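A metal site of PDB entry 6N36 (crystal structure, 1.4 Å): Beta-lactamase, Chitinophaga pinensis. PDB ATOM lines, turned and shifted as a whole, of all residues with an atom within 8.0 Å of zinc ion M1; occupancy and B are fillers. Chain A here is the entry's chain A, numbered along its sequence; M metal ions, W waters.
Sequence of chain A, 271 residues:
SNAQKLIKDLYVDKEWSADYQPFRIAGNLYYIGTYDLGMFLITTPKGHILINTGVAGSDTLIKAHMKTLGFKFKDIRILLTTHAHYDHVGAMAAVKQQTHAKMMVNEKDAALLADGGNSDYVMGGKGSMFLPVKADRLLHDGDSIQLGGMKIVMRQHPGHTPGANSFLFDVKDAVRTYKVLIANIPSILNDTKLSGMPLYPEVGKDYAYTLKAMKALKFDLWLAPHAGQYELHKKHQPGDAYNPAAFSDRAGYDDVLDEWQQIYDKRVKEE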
ATOM      1  N   TRP A  16     -33.056 -11.404 -27.526  1.00  0.00           N
ATOM      2  CA  TRP A  16     -31.749 -11.389 -26.802  1.00  0.00           C
ATOM      3  C   TRP A  16     -31.578 -12.672 -25.983  1.00  0.00           C
ATOM      4  O   TRP A  16     -30.439 -13.116 -25.774  1.00  0.00           O
ATOM      5  CB  TRP A  16     -31.640 -10.173 -25.874  1.00  0.00           C
ATOM      6  CG  TRP A  16     -31.442  -8.882 -26.590  1.00  0.00           C
ATOM      7  CD1 TRP A  16     -31.415  -8.665 -27.932  1.00  0.00           C
ATOM      8  CD2 TRP A  16     -31.330  -7.602 -25.959  1.00  0.00           C
ATOM      9  NE1 TRP A  16     -31.284  -7.318 -28.177  1.00  0.00           N
ATOM     10  CE2 TRP A  16     -31.175  -6.657 -26.986  1.00  0.00           C
ATOM     11  CE3 TRP A  16     -31.351  -7.177 -24.616  1.00  0.00           C
ATOM     12  CZ2 TRP A  16     -31.078  -5.287 -26.694  1.00  0.00           C
ATOM     13  CZ3 TRP A  16     -31.214  -5.836 -24.336  1.00  0.00           C
ATOM     14  CH2 TRP A  16     -31.109  -4.909 -25.377  1.00  0.00           C
ATOM     15  N   THR A  82     -16.972  -6.603 -27.364  1.00  0.00           N
ATOM     16  CA  THR A  82     -17.033  -5.564 -28.404  1.00  0.00           C
ATOM     17  C   THR A  82     -17.373  -4.184 -27.835  1.00  0.00           C
ATOM     18  O   THR A  82     -16.926  -3.168 -28.393  1.00  0.00           O
ATOM     19  CB  THR A  82     -17.959  -5.962 -29.534  1.00  0.00           C
ATOM     20  OG1 THR A  82     -19.270  -6.232 -29.046  1.00  0.00           O
ATOM     21  CG2 THR A  82     -17.436  -7.161 -30.301  1.00  0.00           C
ATOM     22  N   HIS A  83     -18.185  -4.083 -26.819  1.00  0.00           N
ATOM     23  CA  HIS A  83     -18.425  -2.797 -26.104  1.00  0.00           C
ATOM     24  C   HIS A  83     -19.124  -3.067 -24.792  1.00  0.00           C
ATOM     25  O   HIS A  83     -19.955  -3.990 -24.727  1.00  0.00           O
ATOM     26  CB  HIS A  83     -19.204  -1.791 -26.966  1.00  0.00           C
ATOM     27  CG  HIS A  83     -20.639  -2.102 -27.273  1.00  0.00           C
ATOM     28  ND1 HIS A  83     -21.055  -2.717 -28.423  1.00  0.00           N
ATOM     29  CD2 HIS A  83     -21.760  -1.751 -26.627  1.00  0.00           C
ATOM     30  CE1 HIS A  83     -22.381  -2.737 -28.458  1.00  0.00           C
ATOM     31  NE2 HIS A  83     -22.847  -2.145 -27.377  1.00  0.00           N
ATOM     32  N   ALA A  84     -18.943  -2.193 -23.810  1.00  0.00           N
ATOM     33  CA  ALA A  84     -19.443  -2.456 -22.444  1.00  0.00           C
ATOM     34  C   ALA A  84     -20.865  -1.912 -22.235  1.00  0.00           C
ATOM     35  O   ALA A  84     -21.050  -0.980 -21.400  1.00  0.00           O
ATOM     36  CB  ALA A  84     -18.495  -1.900 -21.429  1.00  0.00           C
ATOM     37  N   HIS A  85     -21.818  -2.417 -22.987  1.00  0.00           N
ATOM     38  CA  HIS A  85     -23.259  -2.283 -22.700  1.00  0.00           C
ATOM     39  C   HIS A  85     -23.774  -3.583 -22.104  1.00  0.00           C
ATOM     40  O   HIS A  85     -23.244  -4.667 -22.412  1.00  0.00           O
ATOM     41  CB  HIS A  85     -24.052  -1.912 -23.966  1.00  0.00           C
ATOM     42  CG  HIS A  85     -23.991  -0.471 -24.365  1.00  0.00           C
ATOM     43  ND1 HIS A  85     -24.323  -0.015 -25.648  1.00  0.00           N
ATOM     44  CD2 HIS A  85     -23.599   0.617 -23.666  1.00  0.00           C
ATOM     45  CE1 HIS A  85     -24.194   1.290 -25.675  1.00  0.00           C
ATOM     46  NE2 HIS A  85     -23.767   1.708 -24.479  1.00  0.00           N
ATOM     47  N   TYR A  86     -24.846  -3.501 -21.327  1.00  0.00           N
ATOM     48  CA  TYR A  86     -25.338  -4.643 -20.537  1.00  0.00           C
ATOM     49  C   TYR A  86     -25.776  -5.838 -21.404  1.00  0.00           C
ATOM     50  O   TYR A  86     -25.867  -6.953 -20.844  1.00  0.00           O
ATOM     51  CB  TYR A  86     -26.451  -4.196 -19.592  1.00  0.00           C
ATOM     52  CG  TYR A  86     -27.779  -3.930 -20.252  1.00  0.00           C
ATOM     53  CD1 TYR A  86     -28.059  -2.693 -20.802  1.00  0.00           C
ATOM     54  CD2 TYR A  86     -28.781  -4.883 -20.247  1.00  0.00           C
ATOM     55  CE1 TYR A  86     -29.303  -2.396 -21.353  1.00  0.00           C
ATOM     56  CE2 TYR A  86     -30.043  -4.609 -20.757  1.00  0.00           C
ATOM     57  CZ  TYR A  86     -30.306  -3.357 -21.307  1.00  0.00           C
ATOM     58  OH  TYR A  86     -31.512  -3.069 -21.840  1.00  0.00           O
ATOM     59  N   ASP A  87     -26.139  -5.652 -22.654  1.00  0.00           N
ATOM     60  CA  ASP A  87     -26.523  -6.773 -23.555  1.00  0.00           C
ATOM     61  C   ASP A  87     -25.300  -7.541 -24.063  1.00  0.00           C
ATOM     62  O   ASP A  87     -25.469  -8.630 -24.652  1.00  0.00           O
ATOM     63  CB  ASP A  87     -27.427  -6.296 -24.694  1.00  0.00           C
ATOM     64  CG  ASP A  87     -26.856  -5.206 -25.571  1.00  0.00           C
ATOM     65  OD1 ASP A  87     -26.037  -4.385 -25.029  1.00  0.00           O
ATOM     66  OD2 ASP A  87     -27.281  -5.135 -26.778  1.00  0.00           O
ATOM     67  N   HIS A  88     -24.059  -7.057 -23.856  1.00  0.00           N
ATOM     68  CA  HIS A  88     -22.821  -7.734 -24.281  1.00  0.00           C
ATOM     69  C   HIS A  88     -21.910  -8.089 -23.110  1.00  0.00           C
ATOM     70  O   HIS A  88     -20.969  -8.897 -23.340  1.00  0.00           O
ATOM     71  CB  HIS A  88     -22.061  -6.912 -25.332  1.00  0.00           C
ATOM     72  CG  HIS A  88     -22.991  -6.532 -26.443  1.00  0.00           C
ATOM     73  ND1 HIS A  88     -23.532  -7.459 -27.316  1.00  0.00           N
ATOM     74  CD2 HIS A  88     -23.555  -5.331 -26.724  1.00  0.00           C
ATOM     75  CE1 HIS A  88     -24.407  -6.800 -28.110  1.00  0.00           C
ATOM     76  NE2 HIS A  88     -24.389  -5.484 -27.770  1.00  0.00           N
ATOM     77  N   ASP A 120     -22.167   5.463 -18.066  1.00  0.00           N
ATOM     78  CA  ASP A 120     -22.523   5.413 -19.492  1.00  0.00           C
ATOM     79  C   ASP A 120     -22.980   6.791 -19.983  1.00  0.00           C
ATOM     80  O   ASP A 120     -23.829   7.441 -19.341  1.00  0.00           O
ATOM     81  CB  ASP A 120     -23.605   4.380 -19.736  1.00  0.00           C
ATOM     82  CG  ASP A 120     -23.793   4.120 -21.221  1.00  0.00           C
ATOM     83  OD1 ASP A 120     -24.563   4.885 -21.886  1.00  0.00           O
ATOM     84  OD2 ASP A 120     -23.092   3.216 -21.734  1.00  0.00           O
ATOM     85  N   MET A 123     -26.870   6.238 -20.856  1.00  0.00           N
ATOM     86  CA  MET A 123     -27.762   5.479 -19.952  1.00  0.00           C
ATOM     87  C   MET A 123     -27.292   5.584 -18.507  1.00  0.00           C
ATOM     88  O   MET A 123     -27.927   4.888 -17.667  1.00  0.00           O
ATOM     89  CB  MET A 123     -27.798   3.991 -20.372  1.00  0.00           C
ATOM     90  CG  MET A 123     -28.403   3.791 -21.734  1.00  0.00           C
ATOM     91  SD  MET A 123     -28.351   2.069 -22.287  1.00  0.00           S
ATOM     92  CE  MET A 123     -26.619   1.896 -22.641  1.00  0.00           C
ATOM     93  N   HIS A 160     -20.065   4.263 -30.265  1.00  0.00           N
ATOM     94  CA  HIS A 160     -21.211   3.552 -29.622  1.00  0.00           C
ATOM     95  C   HIS A 160     -20.944   3.438 -28.108  1.00  0.00           C
ATOM     96  O   HIS A 160     -21.824   3.726 -27.301  1.00  0.00           O
ATOM     97  CB  HIS A 160     -21.373   2.203 -30.307  1.00  0.00           C
ATOM     98  CG  HIS A 160     -22.557   1.494 -29.817  1.00  0.00           C
ATOM     99  ND1 HIS A 160     -23.804   1.720 -30.338  1.00  0.00           N
ATOM    100  CD2 HIS A 160     -22.694   0.611 -28.816  1.00  0.00           C
ATOM    101  CE1 HIS A 160     -24.672   1.005 -29.646  1.00  0.00           C
ATOM    102  NE2 HIS A 160     -24.037   0.327 -28.722  1.00  0.00           N
ATOM    103  N   THR A 161     -19.693   3.167 -27.714  1.00  0.00           N
ATOM    104  CA  THR A 161     -19.134   3.471 -26.411  1.00  0.00           C
ATOM    105  C   THR A 161     -17.743   4.033 -26.673  1.00  0.00           C
ATOM    106  O   THR A 161     -17.200   3.810 -27.753  1.00  0.00           O
ATOM    107  CB  THR A 161     -18.986   2.297 -25.446  1.00  0.00           C
ATOM    108  OG1 THR A 161     -18.110   1.346 -26.028  1.00  0.00           O
ATOM    109  CG2 THR A 161     -20.309   1.630 -25.187  1.00  0.00           C
ATOM    110  N   ALA A 164     -15.618   1.033 -27.596  1.00  0.00           N
ATOM    111  CA  ALA A 164     -16.108   0.077 -28.604  1.00  0.00           C
ATOM    112  C   ALA A 164     -14.976  -0.325 -29.537  1.00  0.00           C
ATOM    113  O   ALA A 164     -14.044   0.503 -29.887  1.00  0.00           O
ATOM    114  CB  ALA A 164     -17.289   0.584 -29.363  1.00  0.00           C
ATOM    115  N   ASN A 184     -17.757  -4.256 -34.451  1.00  0.00           N
ATOM    116  CA  ASN A 184     -18.715  -3.464 -33.659  1.00  0.00           C
ATOM    117  C   ASN A 184     -19.267  -2.346 -34.536  1.00  0.00           C
ATOM    118  O   ASN A 184     -18.620  -1.394 -34.801  1.00  0.00           O
ATOM    119  CB  ASN A 184     -18.104  -2.939 -32.368  1.00  0.00           C
ATOM    120  CG  ASN A 184     -19.216  -2.586 -31.414  1.00  0.00           C
ATOM    121  OD1 ASN A 184     -19.721  -3.476 -30.694  1.00  0.00           O
ATOM    122  ND2 ASN A 184     -19.640  -1.306 -31.409  1.00  0.00           N
ATOM    123  N   ILE A 185     -20.506  -2.489 -34.929  1.00  0.00           N
ATOM    124  CA  ILE A 185     -21.135  -1.584 -35.927  1.00  0.00           C
ATOM    125  C   ILE A 185     -21.396  -0.263 -35.204  1.00  0.00           C
ATOM    126  O   ILE A 185     -21.810  -0.228 -34.053  1.00  0.00           O
ATOM    127  CB  ILE A 185     -22.418  -2.217 -36.485  1.00  0.00           C
ATOM    128  CG1 ILE A 185     -22.107  -3.461 -37.327  1.00  0.00           C
ATOM    129  CG2 ILE A 185     -23.245  -1.190 -37.270  1.00  0.00           C
ATOM    130  CD1 ILE A 185     -21.153  -3.282 -38.460  1.00  0.00           C
ATOM    131  N   SER A 187     -23.486   2.012 -34.577  1.00  0.00           N
ATOM    132  CA  SER A 187     -24.859   2.496 -34.382  1.00  0.00           C
ATOM    133  C   SER A 187     -24.894   3.682 -33.422  1.00  0.00           C
ATOM    134  O   SER A 187     -24.124   3.744 -32.490  1.00  0.00           O
ATOM    135  CB  SER A 187     -25.781   1.380 -33.986  1.00  0.00           C
ATOM    136  OG  SER A 187     -25.399   0.854 -32.744  1.00  0.00           O
ATOM    137  N   LEU A 189     -27.344   5.986 -30.911  1.00  0.00           N
ATOM    138  CA  LEU A 189     -28.611   5.942 -30.145  1.00  0.00           C
ATOM    139  C   LEU A 189     -29.327   7.278 -30.364  1.00  0.00           C
ATOM    140  O   LEU A 189     -28.708   8.323 -30.730  1.00  0.00           O
ATOM    141  CB  LEU A 189     -28.341   5.708 -28.664  1.00  0.00           C
ATOM    142  CG  LEU A 189     -27.780   4.325 -28.327  1.00  0.00           C
ATOM    143  CD1 LEU A 189     -27.656   4.161 -26.812  1.00  0.00           C
ATOM    144  CD2 LEU A 189     -28.647   3.248 -28.904  1.00  0.00           C
ATOM    145  N   PRO A 225     -22.243  -8.044 -33.243  1.00  0.00           N
ATOM    146  CA  PRO A 225     -22.846  -8.396 -31.967  1.00  0.00           C
ATOM    147  C   PRO A 225     -24.351  -8.617 -32.011  1.00  0.00           C
ATOM    148  O   PRO A 225     -24.830  -9.191 -31.074  1.00  0.00           O
ATOM    149  CB  PRO A 225     -22.508  -7.206 -31.071  1.00  0.00           C
ATOM    150  CG  PRO A 225     -21.270  -6.617 -31.665  1.00  0.00           C
ATOM    151  CD  PRO A 225     -21.485  -6.768 -33.158  1.00  0.00           C
ATOM    152  N   HIS A 226     -25.040  -8.081 -33.027  1.00  0.00           N
ATOM    153  CA  HIS A 226     -26.490  -8.265 -33.173  1.00  0.00           C
ATOM    154  C   HIS A 226     -26.746  -8.944 -34.514  1.00  0.00           C
ATOM    155  O   HIS A 226     -26.260  -8.467 -35.534  1.00  0.00           O
ATOM    156  CB  HIS A 226     -27.228  -6.934 -33.089  1.00  0.00           C
ATOM    157  CG  HIS A 226     -27.255  -6.380 -31.710  1.00  0.00           C
ATOM    158  ND1 HIS A 226     -28.192  -6.786 -30.741  1.00  0.00           N
ATOM    159  CD2 HIS A 226     -26.424  -5.495 -31.104  1.00  0.00           C
ATOM    160  CE1 HIS A 226     -27.947  -6.124 -29.623  1.00  0.00           C
ATOM    161  NE2 HIS A 226     -26.884  -5.339 -29.796  1.00  0.00           N
ATOM    162  N   GLN A 229     -27.603  -6.874 -37.705  1.00  0.00           N
ATOM    163  CA  GLN A 229     -26.539  -6.007 -38.267  1.00  0.00           C
ATOM    164  C   GLN A 229     -25.858  -6.713 -39.443  1.00  0.00           C
ATOM    165  O   GLN A 229     -25.361  -6.005 -40.315  1.00  0.00           O
ATOM    166  CB  GLN A 229     -25.553  -5.618 -37.181  1.00  0.00           C
ATOM    167  CG  GLN A 229     -26.211  -4.610 -36.267  1.00  0.00           C
ATOM    168  CD  GLN A 229     -25.371  -4.220 -35.092  1.00  0.00           C
ATOM    169  OE1 GLN A 229     -24.552  -5.002 -34.614  1.00  0.00           O
ATOM    170  NE2 GLN A 229     -25.681  -3.006 -34.615  1.00  0.00           N
HETATM  171 ZN    ZN M   1     -24.788  -1.121 -27.370  1.00  0.00          ZN
HETATM  172 ZN    ZN M   2     -26.047  -4.250 -28.245  1.00  0.00          ZN
HETATM  173  O   HOH W   1     -26.800  -0.128 -27.640  1.00  0.00           O
HETATM  174  O   HOH W   2     -26.042  -2.382 -26.386  1.00  0.00           O
HETATM  175  O   HOH W   3     -25.344  -2.611 -29.193  1.00  0.00           O
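A ring nitrogen (NE2) of His 85 is in hydrogen-bond range of the side-chain carboxylate (OD2) of Asp 120 (3.2 Å).
A ring nitrogen (ND1) of His 160 sits at hydrogen-bond distance from the backbone carbonyl oxygen of Ser 187 (3.0 Å).
OD1 of Asn 184 sits at hydrogen-bond distance from ND1 of His 83 (2.7 Å).
Within 4 Å of zinc ion M1: His 83, His 85 and His 160.
Water W2 is bound to zinc ion M1 (2.0 Å).
Zinc ion M1 is bound by a ring nitrogen (ND1) of His 85 (2.1 Å).
Zinc ion M1 is bound by NE2 of His 160 (2.1 Å).
A ring nitrogen (NE2) of His 83 is bound to zinc ion M1 (2.2 Å).
Zinc ion M1 is bound by water W1 (2.3 Å).
Water W3 binds zinc ion M1 (2.4 Å).
Zinc ion M1 has six donor atoms within binding distance.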
